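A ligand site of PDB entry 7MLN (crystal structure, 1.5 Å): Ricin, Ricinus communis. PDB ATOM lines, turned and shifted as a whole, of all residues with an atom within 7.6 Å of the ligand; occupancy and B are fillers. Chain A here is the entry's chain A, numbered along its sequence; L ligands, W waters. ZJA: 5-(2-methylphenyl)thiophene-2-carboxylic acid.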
ATOM      1  N   TYR A 184     -13.766  -9.935  -9.025  1.00  0.00           N
ATOM      2  CA  TYR A 184     -13.719  -9.394  -7.644  1.00  0.00           C
ATOM      3  C   TYR A 184     -15.104  -8.839  -7.282  1.00  0.00           C
ATOM      4  O   TYR A 184     -15.617  -9.172  -6.230  1.00  0.00           O
ATOM      5  CB  TYR A 184     -12.628  -8.342  -7.526  1.00  0.00           C
ATOM      6  CG  TYR A 184     -12.442  -7.797  -6.135  1.00  0.00           C
ATOM      7  CD1 TYR A 184     -11.705  -8.496  -5.185  1.00  0.00           C
ATOM      8  CD2 TYR A 184     -13.029  -6.611  -5.754  1.00  0.00           C
ATOM      9  CE1 TYR A 184     -11.502  -7.987  -3.918  1.00  0.00           C
ATOM     10  CE2 TYR A 184     -12.852  -6.091  -4.473  1.00  0.00           C
ATOM     11  CZ  TYR A 184     -12.104  -6.804  -3.555  1.00  0.00           C
ATOM     12  OH  TYR A 184     -11.913  -6.292  -2.300  1.00  0.00           O
ATOM     13  N   GLU A 188     -18.099 -10.032  -4.687  1.00  0.00           N
ATOM     14  CA  GLU A 188     -18.753  -9.132  -3.690  1.00  0.00           C
ATOM     15  C   GLU A 188     -20.265  -9.327  -3.747  1.00  0.00           C
ATOM     16  O   GLU A 188     -20.904  -9.357  -2.689  1.00  0.00           O
ATOM     17  CB  GLU A 188     -18.407  -7.665  -3.969  1.00  0.00           C
ATOM     18  CG  GLU A 188     -16.955  -7.354  -3.675  1.00  0.00           C
ATOM     19  CD  GLU A 188     -16.675  -7.163  -2.195  1.00  0.00           C
ATOM     20  OE1 GLU A 188     -17.518  -6.543  -1.517  1.00  0.00           O
ATOM     21  OE2 GLU A 188     -15.655  -7.679  -1.741  1.00  0.00           O
ATOM     22  N   ASP A 202     -17.362  -1.232  -0.746  1.00  0.00           N
ATOM     23  CA  ASP A 202     -16.226  -0.642  -0.007  1.00  0.00           C
ATOM     24  C   ASP A 202     -15.272   0.011  -1.002  1.00  0.00           C
ATOM     25  O   ASP A 202     -15.455  -0.077  -2.227  1.00  0.00           O
ATOM     26  CB  ASP A 202     -15.641  -1.686   0.944  1.00  0.00           C
ATOM     27  CG  ASP A 202     -14.739  -2.737   0.308  1.00  0.00           C
ATOM     28  OD1 ASP A 202     -14.118  -2.449  -0.735  1.00  0.00           O
ATOM     29  OD2 ASP A 202     -14.635  -3.828   0.918  1.00  0.00           O
ATOM     30  N   PRO A 203     -14.264   0.767  -0.522  1.00  0.00           N
ATOM     31  CA  PRO A 203     -13.377   1.527  -1.403  1.00  0.00           C
ATOM     32  C   PRO A 203     -12.615   0.670  -2.423  1.00  0.00           C
ATOM     33  O   PRO A 203     -12.272   1.192  -3.469  1.00  0.00           O
ATOM     34  CB  PRO A 203     -12.390   2.209  -0.427  1.00  0.00           C
ATOM     35  CG  PRO A 203     -13.165   2.298   0.853  1.00  0.00           C
ATOM     36  CD  PRO A 203     -13.991   1.037   0.897  1.00  0.00           C
ATOM     37  N   SER A 204     -12.375  -0.607  -2.117  1.00  0.00           N
ATOM     38  CA  SER A 204     -11.692  -1.557  -3.032  1.00  0.00           C
ATOM     39  C   SER A 204     -12.544  -1.722  -4.288  1.00  0.00           C
ATOM     40  O   SER A 204     -12.005  -1.630  -5.384  1.00  0.00           O
ATOM     41  CB  SER A 204     -11.356  -2.876  -2.395  1.00  0.00           C
ATOM     42  OG  SER A 204     -12.480  -3.680  -2.082  1.00  0.00           O
ATOM     43  N   VAL A 205     -13.863  -1.841  -4.105  1.00  0.00           N
ATOM     44  CA  VAL A 205     -14.817  -2.023  -5.242  1.00  0.00           C
ATOM     45  C   VAL A 205     -14.902  -0.712  -6.009  1.00  0.00           C
ATOM     46  O   VAL A 205     -14.841  -0.730  -7.236  1.00  0.00           O
ATOM     47  CB  VAL A 205     -16.187  -2.474  -4.706  1.00  0.00           C
ATOM     48  CG1 VAL A 205     -17.256  -2.461  -5.781  1.00  0.00           C
ATOM     49  CG2 VAL A 205     -16.085  -3.837  -4.050  1.00  0.00           C
ATOM     50  N   THR A 207     -12.838   1.843  -6.252  1.00  0.00           N
ATOM     51  CA  THR A 207     -11.594   2.220  -6.962  1.00  0.00           C
ATOM     52  C   THR A 207     -11.388   1.305  -8.179  1.00  0.00           C
ATOM     53  O   THR A 207     -10.978   1.834  -9.215  1.00  0.00           O
ATOM     54  CB  THR A 207     -10.415   2.301  -5.991  1.00  0.00           C
ATOM     55  OG1 THR A 207     -10.688   3.432  -5.176  1.00  0.00           O
ATOM     56  CG2 THR A 207      -9.087   2.471  -6.700  1.00  0.00           C
ATOM     57  N   LEU A 208     -11.713   0.023  -8.068  1.00  0.00           N
ATOM     58  CA  LEU A 208     -11.695  -0.883  -9.247  1.00  0.00           C
ATOM     59  C   LEU A 208     -12.638  -0.338 -10.330  1.00  0.00           C
ATOM     60  O   LEU A 208     -12.203  -0.183 -11.477  1.00  0.00           O
ATOM     61  CB  LEU A 208     -12.076  -2.290  -8.801  1.00  0.00           C
ATOM     62  CG  LEU A 208     -10.958  -3.079  -8.125  1.00  0.00           C
ATOM     63  CD1 LEU A 208     -11.480  -4.416  -7.627  1.00  0.00           C
ATOM     64  CD2 LEU A 208      -9.767  -3.245  -9.060  1.00  0.00           C
ATOM     65  N   LEU A 215      -6.806   0.494 -16.057  1.00  0.00           N
ATOM     66  CA  LEU A 215      -6.286  -0.901 -15.937  1.00  0.00           C
ATOM     67  C   LEU A 215      -6.275  -1.570 -17.317  1.00  0.00           C
ATOM     68  O   LEU A 215      -5.293  -2.267 -17.626  1.00  0.00           O
ATOM     69  CB  LEU A 215      -7.109  -1.720 -14.952  1.00  0.00           C
ATOM     70  CG  LEU A 215      -6.979  -1.336 -13.476  1.00  0.00           C
ATOM     71  CD1 LEU A 215      -8.088  -1.983 -12.668  1.00  0.00           C
ATOM     72  CD2 LEU A 215      -5.619  -1.724 -12.919  1.00  0.00           C
ATOM     73  N   LEU A 233      -4.487   1.555  -6.631  1.00  0.00           N
ATOM     74  CA  LEU A 233      -5.804   1.002  -6.234  1.00  0.00           C
ATOM     75  C   LEU A 233      -5.961   1.163  -4.724  1.00  0.00           C
ATOM     76  O   LEU A 233      -4.979   1.581  -4.056  1.00  0.00           O
ATOM     77  CB  LEU A 233      -5.878  -0.471  -6.654  1.00  0.00           C
ATOM     78  CG  LEU A 233      -5.729  -0.739  -8.155  1.00  0.00           C
ATOM     79  CD1 LEU A 233      -5.732  -2.226  -8.431  1.00  0.00           C
ATOM     80  CD2 LEU A 233      -6.820  -0.040  -8.957  1.00  0.00           C
ATOM     81  N   GLN A 234      -7.136   0.851  -4.186  1.00  0.00           N
ATOM     82  CA  GLN A 234      -7.442   0.962  -2.740  1.00  0.00           C
ATOM     83  C   GLN A 234      -7.717  -0.421  -2.166  1.00  0.00           C
ATOM     84  O   GLN A 234      -8.340  -1.273  -2.850  1.00  0.00           O
ATOM     85  CB  GLN A 234      -8.661   1.854  -2.498  1.00  0.00           C
ATOM     86  CG  GLN A 234      -8.377   3.344  -2.560  1.00  0.00           C
ATOM     87  CD  GLN A 234      -9.564   4.153  -2.102  1.00  0.00           C
ATOM     88  OE1 GLN A 234      -9.525   4.826  -1.065  1.00  0.00           O
ATOM     89  NE2 GLN A 234     -10.641   4.089  -2.858  1.00  0.00           N
ATOM     90  N   ARG A 235      -7.330  -0.606  -0.907  1.00  0.00           N
ATOM     91  CA  ARG A 235      -7.740  -1.749  -0.073  1.00  0.00           C
ATOM     92  C   ARG A 235      -9.138  -1.460   0.469  1.00  0.00           C
ATOM     93  O   ARG A 235      -9.610  -0.325   0.284  1.00  0.00           O
ATOM     94  CB  ARG A 235      -6.735  -1.942   1.064  1.00  0.00           C
ATOM     95  CG  ARG A 235      -5.329  -2.251   0.577  1.00  0.00           C
ATOM     96  CD  ARG A 235      -4.432  -2.546   1.744  1.00  0.00           C
ATOM     97  NE  ARG A 235      -3.042  -2.705   1.330  1.00  0.00           N
ATOM     98  CZ  ARG A 235      -2.477  -3.870   1.020  1.00  0.00           C
ATOM     99  NH1 ARG A 235      -1.199  -3.888   0.682  1.00  0.00           N
ATOM    100  NH2 ARG A 235      -3.174  -4.999   1.056  1.00  0.00           N
ATOM    101  N   ARG A 236      -9.745  -2.451   1.121  1.00  0.00           N
ATOM    102  CA  ARG A 236     -11.083  -2.337   1.766  1.00  0.00           C
ATOM    103  C   ARG A 236     -11.067  -1.217   2.814  1.00  0.00           C
ATOM    104  O   ARG A 236     -12.137  -0.610   3.041  1.00  0.00           O
ATOM    105  CB  ARG A 236     -11.495  -3.634   2.444  1.00  0.00           C
ATOM    106  CG  ARG A 236     -11.701  -4.800   1.479  1.00  0.00           C
ATOM    107  CD  ARG A 236     -12.378  -5.939   2.184  1.00  0.00           C
ATOM    108  NE  ARG A 236     -12.343  -7.167   1.418  1.00  0.00           N
ATOM    109  CZ  ARG A 236     -13.178  -7.497   0.435  1.00  0.00           C
ATOM    110  NH1 ARG A 236     -14.169  -6.683   0.078  1.00  0.00           N
ATOM    111  NH2 ARG A 236     -13.026  -8.653  -0.192  1.00  0.00           N
ATOM    112  N   ASN A 237      -9.914  -0.948   3.444  1.00  0.00           N
ATOM    113  CA  ASN A 237      -9.807   0.085   4.513  1.00  0.00           C
ATOM    114  C   ASN A 237      -9.499   1.464   3.903  1.00  0.00           C
ATOM    115  O   ASN A 237      -9.370   2.401   4.680  1.00  0.00           O
ATOM    116  CB  ASN A 237      -8.785  -0.309   5.578  1.00  0.00           C
ATOM    117  CG  ASN A 237      -7.335  -0.266   5.112  1.00  0.00           C
ATOM    118  OD1 ASN A 237      -7.023   0.159   4.009  1.00  0.00           O
ATOM    119  ND2 ASN A 237      -6.432  -0.683   5.987  1.00  0.00           N
ATOM    120  N   GLY A 238      -9.414   1.580   2.572  1.00  0.00           N
ATOM    121  CA  GLY A 238      -9.234   2.851   1.857  1.00  0.00           C
ATOM    122  C   GLY A 238      -7.773   3.220   1.620  1.00  0.00           C
ATOM    123  O   GLY A 238      -7.530   4.195   0.891  1.00  0.00           O
ATOM    124  N   SER A 239      -6.813   2.482   2.195  1.00  0.00           N
ATOM    125  CA  SER A 239      -5.368   2.744   1.983  1.00  0.00           C
ATOM    126  C   SER A 239      -5.002   2.425   0.521  1.00  0.00           C
ATOM    127  O   SER A 239      -5.635   1.508  -0.053  1.00  0.00           O
ATOM    128  CB  SER A 239      -4.511   1.979   2.968  1.00  0.00           C
ATOM    129  OG  SER A 239      -4.684   0.583   2.831  1.00  0.00           O
ATOM    130  N   PHE A 241      -2.393   1.278  -2.602  1.00  0.00           N
ATOM    131  CA  PHE A 241      -1.185   0.519  -3.014  1.00  0.00           C
ATOM    132  C   PHE A 241      -1.018   0.669  -4.523  1.00  0.00           C
ATOM    133  O   PHE A 241      -1.983   1.005  -5.228  1.00  0.00           O
ATOM    134  CB  PHE A 241      -1.277  -0.943  -2.579  1.00  0.00           C
ATOM    135  CG  PHE A 241      -2.386  -1.714  -3.224  1.00  0.00           C
ATOM    136  CD1 PHE A 241      -3.653  -1.724  -2.666  1.00  0.00           C
ATOM    137  CD2 PHE A 241      -2.170  -2.408  -4.407  1.00  0.00           C
ATOM    138  CE1 PHE A 241      -4.689  -2.434  -3.267  1.00  0.00           C
ATOM    139  CE2 PHE A 241      -3.206  -3.127  -5.001  1.00  0.00           C
ATOM    140  CZ  PHE A 241      -4.458  -3.127  -4.431  1.00  0.00           C
ATOM    141  N   VAL A 243       0.157  -0.981  -8.301  1.00  0.00           N
ATOM    142  CA  VAL A 243       0.239  -2.221  -9.129  1.00  0.00           C
ATOM    143  C   VAL A 243       1.190  -1.915 -10.299  1.00  0.00           C
ATOM    144  O   VAL A 243       1.005  -0.876 -10.943  1.00  0.00           O
ATOM    145  CB  VAL A 243      -1.142  -2.692  -9.617  1.00  0.00           C
ATOM    146  CG1 VAL A 243      -1.035  -3.967 -10.439  1.00  0.00           C
ATOM    147  CG2 VAL A 243      -2.115  -2.890  -8.458  1.00  0.00           C
ATOM    148  N   ILE A 248      -1.121  -9.881 -10.537  1.00  0.00           N
ATOM    149  CA  ILE A 248      -2.028  -9.776  -9.353  1.00  0.00           C
ATOM    150  C   ILE A 248      -3.450  -9.468  -9.835  1.00  0.00           C
ATOM    151  O   ILE A 248      -4.400  -9.740  -9.068  1.00  0.00           O
ATOM    152  CB  ILE A 248      -1.504  -8.734  -8.342  1.00  0.00           C
ATOM    153  CG1 ILE A 248      -2.119  -8.907  -6.952  1.00  0.00           C
ATOM    154  CG2 ILE A 248      -1.656  -7.314  -8.850  1.00  0.00           C
ATOM    155  CD1 ILE A 248      -1.587 -10.085  -6.167  1.00  0.00           C
ATOM    156  N   LEU A 249      -3.614  -8.952 -11.044  1.00  0.00           N
ATOM    157  CA  LEU A 249      -4.942  -8.528 -11.588  1.00  0.00           C
ATOM    158  C   LEU A 249      -5.647  -9.662 -12.336  1.00  0.00           C
ATOM    159  O   LEU A 249      -6.851  -9.516 -12.584  1.00  0.00           O
ATOM    160  CB  LEU A 249      -4.749  -7.303 -12.486  1.00  0.00           C
ATOM    161  CG  LEU A 249      -4.258  -6.056 -11.762  1.00  0.00           C
ATOM    162  CD1 LEU A 249      -3.864  -4.975 -12.754  1.00  0.00           C
ATOM    163  CD2 LEU A 249      -5.307  -5.547 -10.781  1.00  0.00           C
ATOM    164  N   ILE A 250      -4.975 -10.758 -12.701  1.00  0.00           N
ATOM    165  CA  ILE A 250      -5.613 -11.825 -13.540  1.00  0.00           C
ATOM    166  C   ILE A 250      -6.843 -12.394 -12.829  1.00  0.00           C
ATOM    167  O   ILE A 250      -7.865 -12.617 -13.478  1.00  0.00           O
ATOM    168  CB  ILE A 250      -4.571 -12.890 -13.952  1.00  0.00           C
ATOM    169  CG1 ILE A 250      -3.611 -12.321 -14.988  1.00  0.00           C
ATOM    170  CG2 ILE A 250      -5.251 -14.165 -14.461  1.00  0.00           C
ATOM    171  CD1 ILE A 250      -2.301 -13.064 -15.091  1.00  0.00           C
ATOM    172  N   PRO A 251      -6.838 -12.632 -11.502  1.00  0.00           N
ATOM    173  CA  PRO A 251      -8.028 -13.100 -10.793  1.00  0.00           C
ATOM    174  C   PRO A 251      -9.082 -12.008 -10.507  1.00  0.00           C
ATOM    175  O   PRO A 251     -10.141 -12.363 -10.019  1.00  0.00           O
ATOM    176  CB  PRO A 251      -7.498 -13.641  -9.462  1.00  0.00           C
ATOM    177  CG  PRO A 251      -5.987 -13.647  -9.605  1.00  0.00           C
ATOM    178  CD  PRO A 251      -5.669 -12.563 -10.611  1.00  0.00           C
ATOM    179  N   ILE A 252      -8.763 -10.740 -10.777  1.00  0.00           N
ATOM    180  CA  ILE A 252      -9.558  -9.550 -10.348  1.00  0.00           C
ATOM    181  C   ILE A 252     -10.415  -9.061 -11.512  1.00  0.00           C
ATOM    182  O   ILE A 252     -11.635  -8.800 -11.270  1.00  0.00           O
ATOM    183  CB  ILE A 252      -8.626  -8.424  -9.841  1.00  0.00           C
ATOM    184  CG1 ILE A 252      -7.761  -8.845  -8.655  1.00  0.00           C
ATOM    185  CG2 ILE A 252      -9.433  -7.163  -9.530  1.00  0.00           C
ATOM    186  CD1 ILE A 252      -8.510  -9.110  -7.366  1.00  0.00           C
ATOM    187  N   ILE A 253      -9.805  -8.883 -12.690  1.00  0.00           N
ATOM    188  CA  ILE A 253     -10.431  -8.245 -13.888  1.00  0.00           C
ATOM    189  C   ILE A 253     -10.742  -9.315 -14.944  1.00  0.00           C
ATOM    190  O   ILE A 253      -9.845 -10.073 -15.346  1.00  0.00           O
ATOM    191  CB  ILE A 253      -9.586  -7.069 -14.433  1.00  0.00           C
ATOM    192  CG1 ILE A 253     -10.334  -6.311 -15.533  1.00  0.00           C
ATOM    193  CG2 ILE A 253      -8.214  -7.494 -14.921  1.00  0.00           C
ATOM    194  CD1 ILE A 253      -9.766  -4.937 -15.810  1.00  0.00           C
HETATM  195  C12 ZJA L   1      -7.314  -5.241   1.381  1.00  0.00           C
HETATM  196  C15 ZJA L   1      -8.115  -4.396  -5.485  1.00  0.00           C
HETATM  197  C01 ZJA L   1      -5.589  -6.495  -6.847  1.00  0.00           C
HETATM  198  C02 ZJA L   1      -6.483  -5.655  -6.740  1.00  0.00           C
HETATM  199  C03 ZJA L   1      -7.153  -5.328  -5.530  1.00  0.00           C
HETATM  200  C04 ZJA L   1      -6.743  -6.085  -4.261  1.00  0.00           C
HETATM  201  C05 ZJA L   1      -5.729  -6.952  -4.700  1.00  0.00           C
HETATM  202  C06 ZJA L   1      -5.163  -7.224  -5.767  1.00  0.00           C
HETATM  203  C07 ZJA L   1      -7.359  -5.830  -3.027  1.00  0.00           C
HETATM  204  C08 ZJA L   1      -8.725  -5.621  -2.741  1.00  0.00           C
HETATM  205  C09 ZJA L   1      -8.699  -5.420  -1.334  1.00  0.00           C
HETATM  206  C10 ZJA L   1      -7.720  -5.445  -0.562  1.00  0.00           C
HETATM  207  S11 ZJA L   1      -6.354  -5.772  -1.502  1.00  0.00           S
HETATM  208  O13 ZJA L   1      -6.149  -5.514   1.424  1.00  0.00           O
HETATM  209  O14 ZJA L   1      -8.382  -4.942   1.801  1.00  0.00           O
HETATM  210  O   HOH W   1      -9.182  -6.729   3.530  1.00  0.00           O
HETATM  211  O   HOH W   2      -8.022  -3.428   4.008  1.00  0.00           O
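O14 of the ligand is in hydrogen-bond range of N of Arg 236, 2.9 Å away.
O13 of the ligand is in salt-bridge range of NH2 of Arg 235.
Merely in contact with the ligand: Tyr 184 (3.3 Å), Ser 204 (3.8 Å), Leu 208 (3.99 Å), Leu 233 (3.9 Å), Phe 241 (3.6 Å), Ile 248 (3.7 Å) and Ile 252 (3.7 Å).
The nearest printed residue that does not touch the ligand is Leu 249 (4.1 Å).
The side-chain hydroxyl (OG) of Ser 204 lies within hydrogen-bond range of the side-chain carboxylate (OD1) of Asp 202, 2.5 Å away.
The guanidinium group of Arg 236 lies within salt-bridge range of the side-chain carboxylate of Glu 188.
OH of Tyr 184 sits at hydrogen-bond distance from OG of Ser 204, 2.7 Å away.
N of Tyr 184 lies within hydrogen-bond range of O of Ile 252.
O of Phe 241 lies within hydrogen-bond range of N of Leu 233 (2.9 Å).
The guanidinium group (NH1) of Arg 236 lies close to the side-chain hydroxyl (OH) of Tyr 184 (3.3 Å).
The guanidinium group (NH1) of Arg 236 lies within salt-bridge range of the side-chain carboxylate (OD2) of Asp 202, at 3.0 Å.
Water W2 lies within hydrogen-bond range of O14 of the ligand and N of Asn 237.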
